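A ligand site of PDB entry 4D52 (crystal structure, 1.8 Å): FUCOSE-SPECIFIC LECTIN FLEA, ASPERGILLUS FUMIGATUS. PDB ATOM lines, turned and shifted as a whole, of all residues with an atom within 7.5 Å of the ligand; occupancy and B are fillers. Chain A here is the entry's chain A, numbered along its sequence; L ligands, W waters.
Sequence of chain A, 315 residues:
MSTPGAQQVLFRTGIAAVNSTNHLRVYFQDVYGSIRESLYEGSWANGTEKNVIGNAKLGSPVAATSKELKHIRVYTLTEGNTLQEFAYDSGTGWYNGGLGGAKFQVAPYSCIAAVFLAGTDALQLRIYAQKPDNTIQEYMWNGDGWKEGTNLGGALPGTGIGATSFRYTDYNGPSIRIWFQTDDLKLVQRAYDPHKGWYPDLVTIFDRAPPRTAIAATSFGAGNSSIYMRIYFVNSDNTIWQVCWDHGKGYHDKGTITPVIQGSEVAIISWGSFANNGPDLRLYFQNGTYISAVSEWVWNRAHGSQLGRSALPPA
OE1 of Glu 37 sits at hydrogen-bond distance from O2 of the ligand (2.6 Å). The guanidinium group of Arg 25 lies within hydrogen-bond range of an oxygen (O3) of the ligand (2.8 Å). O5 of the ligand lies within hydrogen-bond range of O of Leu 69 (2.8 Å). NE1 of Trp 94 lies within hydrogen-bond range of O2 of the ligand (2.8 Å).
The side-chain carboxylate (OE2) of Glu 37 lies within hydrogen-bond range of the side-chain hydroxyl (OH) of Tyr 27 (2.7 Å). The backbone carbonyl oxygen (O) of Asn 51 is in hydrogen-bond range of the backbone NH (N) of Glu 37 (3.0 Å). NH2 of Arg 25 lies within salt-bridge range of OE2 of Glu 41 (2.8 Å). The backbone carbonyl oxygen (O) of Val 18 lies within hydrogen-bond range of the backbone NH (N) of Arg 25. O of Tyr 88 sits at hydrogen-bond distance from N of Ile 72, at 2.8 Å.
Leu 39 touches the ligand (CD2 to O1, 3.4 Å). Ile 72 touches the ligand. CE1 of Tyr 88 touches C6 of the ligand (3.5 Å). Of the 21 residues printed, 7 come within 4 Å of the ligand.
Water W2 lies within hydrogen-bond range of an oxygen (O5) of the ligand and the guanidinium group (NH2) of Arg 25. Water W4 lies within hydrogen-bond range of OG of Ser 90 (2.5 Å), OH of Tyr 88 (2.9 Å) and O5 of the ligand (3.0 Å).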
ATOM      1  N   VAL A  18      21.446 -12.372  13.364  1.00  0.00           N
ATOM      2  CA  VAL A  18      21.595 -12.456  11.918  1.00  0.00           C
ATOM      3  C   VAL A  18      21.075 -11.200  11.232  1.00  0.00           C
ATOM      4  O   VAL A  18      20.388 -10.381  11.826  1.00  0.00           O
ATOM      5  CB  VAL A  18      20.888 -13.686  11.318  1.00  0.00           C
ATOM      6  CG1 VAL A  18      21.453 -14.962  11.926  1.00  0.00           C
ATOM      7  CG2 VAL A  18      19.393 -13.616  11.501  1.00  0.00           C
ATOM      8  N   LEU A  24      17.608  -6.742  10.718  1.00  0.00           N
ATOM      9  CA  LEU A  24      18.278  -7.459  11.817  1.00  0.00           C
ATOM     10  C   LEU A  24      17.333  -8.413  12.550  1.00  0.00           C
ATOM     11  O   LEU A  24      16.155  -8.096  12.759  1.00  0.00           O
ATOM     12  CB  LEU A  24      18.851  -6.477  12.839  1.00  0.00           C
ATOM     13  CG  LEU A  24      19.445  -5.152  12.323  1.00  0.00           C
ATOM     14  CD1 LEU A  24      19.843  -4.263  13.495  1.00  0.00           C
ATOM     15  CD2 LEU A  24      20.632  -5.422  11.420  1.00  0.00           C
ATOM     16  N   ARG A  25      17.876  -9.535  12.990  1.00  0.00           N
ATOM     17  CA  ARG A  25      17.149 -10.423  13.905  1.00  0.00           C
ATOM     18  C   ARG A  25      18.068 -10.780  15.076  1.00  0.00           C
ATOM     19  O   ARG A  25      19.251 -11.025  14.872  1.00  0.00           O
ATOM     20  CB  ARG A  25      16.683 -11.711  13.198  1.00  0.00           C
ATOM     21  CG  ARG A  25      15.816 -11.504  11.959  1.00  0.00           C
ATOM     22  CD  ARG A  25      14.453 -10.904  12.303  1.00  0.00           C
ATOM     23  NE  ARG A  25      13.606 -10.742  11.121  1.00  0.00           N
ATOM     24  CZ  ARG A  25      13.581  -9.661  10.328  1.00  0.00           C
ATOM     25  NH1 ARG A  25      14.340  -8.593  10.561  1.00  0.00           N
ATOM     26  NH2 ARG A  25      12.781  -9.651   9.270  1.00  0.00           N
ATOM     27  N   TYR A  27      18.231 -13.266  18.642  1.00  0.00           N
ATOM     28  CA  TYR A  27      17.672 -14.419  19.344  1.00  0.00           C
ATOM     29  C   TYR A  27      18.236 -14.459  20.751  1.00  0.00           C
ATOM     30  O   TYR A  27      19.422 -14.210  20.967  1.00  0.00           O
ATOM     31  CB  TYR A  27      17.999 -15.716  18.589  1.00  0.00           C
ATOM     32  CG  TYR A  27      17.516 -15.637  17.183  1.00  0.00           C
ATOM     33  CD1 TYR A  27      16.173 -15.836  16.868  1.00  0.00           C
ATOM     34  CD2 TYR A  27      18.372 -15.280  16.150  1.00  0.00           C
ATOM     35  CE1 TYR A  27      15.700 -15.678  15.586  1.00  0.00           C
ATOM     36  CE2 TYR A  27      17.898 -15.140  14.844  1.00  0.00           C
ATOM     37  CZ  TYR A  27      16.561 -15.322  14.591  1.00  0.00           C
ATOM     38  OH  TYR A  27      16.044 -15.144  13.341  1.00  0.00           O
ATOM     39  N   GLU A  37      12.608 -14.252  19.267  1.00  0.00           N
ATOM     40  CA  GLU A  37      13.194 -13.429  18.213  1.00  0.00           C
ATOM     41  C   GLU A  37      12.703 -12.001  18.352  1.00  0.00           C
ATOM     42  O   GLU A  37      11.480 -11.763  18.361  1.00  0.00           O
ATOM     43  CB  GLU A  37      12.797 -13.938  16.824  1.00  0.00           C
ATOM     44  CG  GLU A  37      13.423 -13.156  15.653  1.00  0.00           C
ATOM     45  CD  GLU A  37      12.812 -13.562  14.320  1.00  0.00           C
ATOM     46  OE1 GLU A  37      11.587 -13.366  14.200  1.00  0.00           O
ATOM     47  OE2 GLU A  37      13.514 -14.134  13.444  1.00  0.00           O
ATOM     48  N   SER A  38      13.651 -11.082  18.481  1.00  0.00           N
ATOM     49  CA  SER A  38      13.416  -9.655  18.294  1.00  0.00           C
ATOM     50  C   SER A  38      13.904  -9.223  16.918  1.00  0.00           C
ATOM     51  O   SER A  38      14.795  -9.857  16.319  1.00  0.00           O
ATOM     52  CB  SER A  38      14.138  -8.862  19.369  1.00  0.00           C
ATOM     53  OG  SER A  38      13.568  -9.151  20.646  1.00  0.00           O
ATOM     54  N   LEU A  39      13.340  -8.159  16.373  1.00  0.00           N
ATOM     55  CA  LEU A  39      13.705  -7.781  15.018  1.00  0.00           C
ATOM     56  C   LEU A  39      13.803  -6.285  14.838  1.00  0.00           C
ATOM     57  O   LEU A  39      13.226  -5.515  15.630  1.00  0.00           O
ATOM     58  CB  LEU A  39      12.769  -8.416  13.989  1.00  0.00           C
ATOM     59  CG  LEU A  39      11.333  -7.961  13.713  1.00  0.00           C
ATOM     60  CD1 LEU A  39      11.229  -6.550  13.139  1.00  0.00           C
ATOM     61  CD2 LEU A  39      10.722  -8.935  12.704  1.00  0.00           C
ATOM     62  N   GLU A  41      13.337  -3.774  11.653  1.00  0.00           N
ATOM     63  CA  GLU A  41      12.909  -3.488  10.297  1.00  0.00           C
ATOM     64  C   GLU A  41      12.479  -2.030  10.300  1.00  0.00           C
ATOM     65  O   GLU A  41      11.282  -1.720  10.371  1.00  0.00           O
ATOM     66  CB  GLU A  41      11.754  -4.404   9.869  1.00  0.00           C
ATOM     67  CG  GLU A  41      12.156  -5.851   9.633  1.00  0.00           C
ATOM     68  CD  GLU A  41      13.059  -6.058   8.412  1.00  0.00           C
ATOM     69  OE1 GLU A  41      13.277  -5.112   7.614  1.00  0.00           O
ATOM     70  OE2 GLU A  41      13.560  -7.171   8.243  1.00  0.00           O
ATOM     71  N   ASN A  46       8.976  -6.973  18.584  1.00  0.00           N
ATOM     72  CA  ASN A  46       8.831  -8.414  18.855  1.00  0.00           C
ATOM     73  C   ASN A  46       9.537  -8.823  20.134  1.00  0.00           C
ATOM     74  O   ASN A  46       9.460  -8.067  21.115  1.00  0.00           O
ATOM     75  CB  ASN A  46       9.192  -9.273  17.629  1.00  0.00           C
ATOM     76  CG  ASN A  46       8.261  -9.037  16.447  1.00  0.00           C
ATOM     77  OD1 ASN A  46       8.570  -9.435  15.322  1.00  0.00           O
ATOM     78  ND2 ASN A  46       7.126  -8.455  16.689  1.00  0.00           N
ATOM     79  N   ASN A  51       6.677 -14.528  20.019  1.00  0.00           N
ATOM     80  CA  ASN A  51       7.772 -14.604  19.071  1.00  0.00           C
ATOM     81  C   ASN A  51       8.722 -15.747  19.418  1.00  0.00           C
ATOM     82  O   ASN A  51       9.920 -15.670  19.211  1.00  0.00           O
ATOM     83  CB  ASN A  51       8.481 -13.260  19.034  1.00  0.00           C
ATOM     84  CG  ASN A  51       7.526 -12.127  18.707  1.00  0.00           C
ATOM     85  OD1 ASN A  51       7.267 -11.244  19.532  1.00  0.00           O
ATOM     86  ND2 ASN A  51       6.924 -12.189  17.517  1.00  0.00           N
ATOM     87  N   ILE A  53      10.314 -19.285  18.850  1.00  0.00           N
ATOM     88  CA  ILE A  53      10.658 -20.174  17.728  1.00  0.00           C
ATOM     89  C   ILE A  53      10.955 -21.612  18.179  1.00  0.00           C
ATOM     90  O   ILE A  53      11.150 -22.506  17.341  1.00  0.00           O
ATOM     91  CB  ILE A  53      11.826 -19.621  16.854  1.00  0.00           C
ATOM     92  CG1 ILE A  53      13.112 -19.459  17.664  1.00  0.00           C
ATOM     93  CG2 ILE A  53      11.414 -18.291  16.220  1.00  0.00           C
ATOM     94  CD1 ILE A  53      14.360 -19.245  16.824  1.00  0.00           C
ATOM     95  N   GLU A  68      21.063 -13.996   3.876  1.00  0.00           N
ATOM     96  CA  GLU A  68      20.251 -12.788   4.011  1.00  0.00           C
ATOM     97  C   GLU A  68      19.241 -13.062   5.132  1.00  0.00           C
ATOM     98  O   GLU A  68      19.649 -13.550   6.195  1.00  0.00           O
ATOM     99  CB  GLU A  68      19.580 -12.431   2.681  1.00  0.00           C
ATOM    100  CG  GLU A  68      20.537 -12.354   1.500  1.00  0.00           C
ATOM    101  CD  GLU A  68      21.663 -11.373   1.685  1.00  0.00           C
ATOM    102  OE1 GLU A  68      21.579 -10.422   2.497  1.00  0.00           O
ATOM    103  OE2 GLU A  68      22.677 -11.553   0.986  1.00  0.00           O
ATOM    104  N   LEU A  69      17.945 -12.738   4.931  1.00  0.00           N
ATOM    105  CA  LEU A  69      16.896 -13.206   5.828  1.00  0.00           C
ATOM    106  C   LEU A  69      15.931 -14.152   5.127  1.00  0.00           C
ATOM    107  O   LEU A  69      14.813 -14.329   5.571  1.00  0.00           O
ATOM    108  CB  LEU A  69      16.175 -12.036   6.495  1.00  0.00           C
ATOM    109  CG  LEU A  69      17.064 -11.154   7.370  1.00  0.00           C
ATOM    110  CD1 LEU A  69      16.235 -10.003   7.929  1.00  0.00           C
ATOM    111  CD2 LEU A  69      17.731 -11.907   8.512  1.00  0.00           C
ATOM    112  N   LYS A  70      16.399 -14.791   4.049  1.00  0.00           N
ATOM    113  CA  LYS A  70      15.616 -15.784   3.310  1.00  0.00           C
ATOM    114  C   LYS A  70      15.674 -17.162   3.973  1.00  0.00           C
ATOM    115  O   LYS A  70      14.708 -17.931   3.943  1.00  0.00           O
ATOM    116  CB  LYS A  70      16.117 -15.911   1.889  1.00  0.00           C
ATOM    117  CG  LYS A  70      15.333 -16.889   1.024  1.00  0.00           C
ATOM    118  CD  LYS A  70      15.887 -16.920  -0.387  1.00  0.00           C
ATOM    119  CE  LYS A  70      15.054 -17.868  -1.267  1.00  0.00           C
ATOM    120  NZ  LYS A  70      15.741 -18.004  -2.572  1.00  0.00           N
ATOM    121  N   HIS A  71      16.830 -17.470   4.533  1.00  0.00           N
ATOM    122  CA  HIS A  71      17.077 -18.727   5.238  1.00  0.00           C
ATOM    123  C   HIS A  71      17.765 -18.422   6.565  1.00  0.00           C
ATOM    124  O   HIS A  71      18.859 -17.859   6.568  1.00  0.00           O
ATOM    125  CB  HIS A  71      17.957 -19.634   4.405  1.00  0.00           C
ATOM    126  CG  HIS A  71      17.420 -19.933   3.037  1.00  0.00           C
ATOM    127  ND1 HIS A  71      16.320 -20.739   2.826  1.00  0.00           N
ATOM    128  CD2 HIS A  71      17.851 -19.551   1.811  1.00  0.00           C
ATOM    129  CE1 HIS A  71      16.078 -20.816   1.528  1.00  0.00           C
ATOM    130  NE2 HIS A  71      17.006 -20.118   0.892  1.00  0.00           N
ATOM    131  N   ILE A  72      17.126 -18.737   7.675  1.00  0.00           N
ATOM    132  CA  ILE A  72      17.745 -18.537   8.983  1.00  0.00           C
ATOM    133  C   ILE A  72      17.788 -19.885   9.708  1.00  0.00           C
ATOM    134  O   ILE A  72      16.849 -20.679   9.612  1.00  0.00           O
ATOM    135  CB  ILE A  72      16.974 -17.506   9.836  1.00  0.00           C
ATOM    136  CG1 ILE A  72      16.845 -16.165   9.108  1.00  0.00           C
ATOM    137  CG2 ILE A  72      17.659 -17.300  11.181  1.00  0.00           C
ATOM    138  CD1 ILE A  72      15.794 -15.246   9.707  1.00  0.00           C
ATOM    139  N   TYR A  88      14.071 -21.312   9.520  1.00  0.00           N
ATOM    140  CA  TYR A  88      13.129 -20.427   8.824  1.00  0.00           C
ATOM    141  C   TYR A  88      13.529 -20.373   7.364  1.00  0.00           C
ATOM    142  O   TYR A  88      14.698 -20.075   7.045  1.00  0.00           O
ATOM    143  CB  TYR A  88      13.155 -19.003   9.404  1.00  0.00           C
ATOM    144  CG  TYR A  88      12.301 -18.042   8.612  1.00  0.00           C
ATOM    145  CD1 TYR A  88      12.818 -17.377   7.502  1.00  0.00           C
ATOM    146  CD2 TYR A  88      10.961 -17.844   8.932  1.00  0.00           C
ATOM    147  CE1 TYR A  88      12.038 -16.530   6.747  1.00  0.00           C
ATOM    148  CE2 TYR A  88      10.163 -16.971   8.180  1.00  0.00           C
ATOM    149  CZ  TYR A  88      10.720 -16.327   7.092  1.00  0.00           C
ATOM    150  OH  TYR A  88       9.945 -15.480   6.329  1.00  0.00           O
ATOM    151  N   ASP A  89      12.570 -20.657   6.482  1.00  0.00           N
ATOM    152  CA  ASP A  89      12.711 -20.308   5.069  1.00  0.00           C
ATOM    153  C   ASP A  89      11.548 -19.403   4.618  1.00  0.00           C
ATOM    154  O   ASP A  89      10.385 -19.612   5.013  1.00  0.00           O
ATOM    155  CB  ASP A  89      12.739 -21.537   4.148  1.00  0.00           C
ATOM    156  CG  ASP A  89      13.780 -22.570   4.538  1.00  0.00           C
ATOM    157  OD1 ASP A  89      14.964 -22.200   4.700  1.00  0.00           O
ATOM    158  OD2 ASP A  89      13.405 -23.774   4.642  1.00  0.00           O
ATOM    159  N   SER A  90      11.863 -18.421   3.772  1.00  0.00           N
ATOM    160  CA  SER A  90      10.823 -17.595   3.169  1.00  0.00           C
ATOM    161  C   SER A  90       9.839 -18.478   2.437  1.00  0.00           C
ATOM    162  O   SER A  90      10.239 -19.343   1.645  1.00  0.00           O
ATOM    163  CB  SER A  90      11.375 -16.555   2.195  1.00  0.00           C
ATOM    164  OG  SER A  90      12.276 -15.704   2.857  1.00  0.00           O
ATOM    165  N   GLY A  93       8.127 -20.439   6.630  1.00  0.00           N
ATOM    166  CA  GLY A  93       8.039 -20.043   8.028  1.00  0.00           C
ATOM    167  C   GLY A  93       8.980 -20.886   8.862  1.00  0.00           C
ATOM    168  O   GLY A  93       9.945 -21.469   8.329  1.00  0.00           O
ATOM    169  N   TRP A  94       8.712 -20.924  10.168  1.00  0.00           N
ATOM    170  CA  TRP A  94       9.562 -21.620  11.139  1.00  0.00           C
ATOM    171  C   TRP A  94       9.173 -23.089  11.295  1.00  0.00           C
ATOM    172  O   TRP A  94       7.990 -23.422  11.296  1.00  0.00           O
ATOM    173  CB  TRP A  94       9.525 -20.967  12.518  1.00  0.00           C
ATOM    174  CG  TRP A  94      10.251 -19.661  12.580  1.00  0.00           C
ATOM    175  CD1 TRP A  94       9.693 -18.411  12.481  1.00  0.00           C
ATOM    176  CD2 TRP A  94      11.660 -19.462  12.760  1.00  0.00           C
ATOM    177  NE1 TRP A  94      10.672 -17.450  12.582  1.00  0.00           N
ATOM    178  CE2 TRP A  94      11.889 -18.068  12.752  1.00  0.00           C
ATOM    179  CE3 TRP A  94      12.756 -20.325  12.900  1.00  0.00           C
ATOM    180  CZ2 TRP A  94      13.162 -17.519  12.867  1.00  0.00           C
ATOM    181  CZ3 TRP A  94      14.022 -19.763  13.034  1.00  0.00           C
ATOM    182  CH2 TRP A  94      14.219 -18.374  13.020  1.00  0.00           C
HETATM  183  C1  LIG L   1       9.861 -11.926   9.696  1.00  0.00           C
HETATM  184  C2  LIG L   1       9.856 -12.632  11.047  1.00  0.00           C
HETATM  185  C3  LIG L   1      10.375 -14.069  10.958  1.00  0.00           C
HETATM  186  C4  LIG L   1      11.744 -14.059  10.259  1.00  0.00           C
HETATM  187  C5  LIG L   1      11.615 -13.361   8.901  1.00  0.00           C
HETATM  188  C6  LIG L   1      12.924 -13.401   8.156  1.00  0.00           C
HETATM  189  O1  LIG L   1       9.538 -10.562   9.951  1.00  0.00           O
HETATM  190  O2  LIG L   1      10.415 -14.630  12.304  1.00  0.00           O
HETATM  191  O3  LIG L   1      12.725 -13.369  11.041  1.00  0.00           O
HETATM  192  O4  LIG L   1      11.146 -12.032   9.107  1.00  0.00           O
HETATM  193  O5  LIG L   1      12.769 -12.888   6.834  1.00  0.00           O
HETATM  194  O6  LIG L   1       8.539 -12.594  11.605  1.00  0.00           O
HETATM  195  O   HOH W   1       9.609  -9.499   7.467  1.00  0.00           O
HETATM  196  O   HOH W   2      11.859 -10.351   6.133  1.00  0.00           O
HETATM  197  O   HOH W   3       6.643 -14.297  10.847  1.00  0.00           O
HETATM  198  O   HOH W   4      11.377 -13.895   4.352  1.00  0.00           O
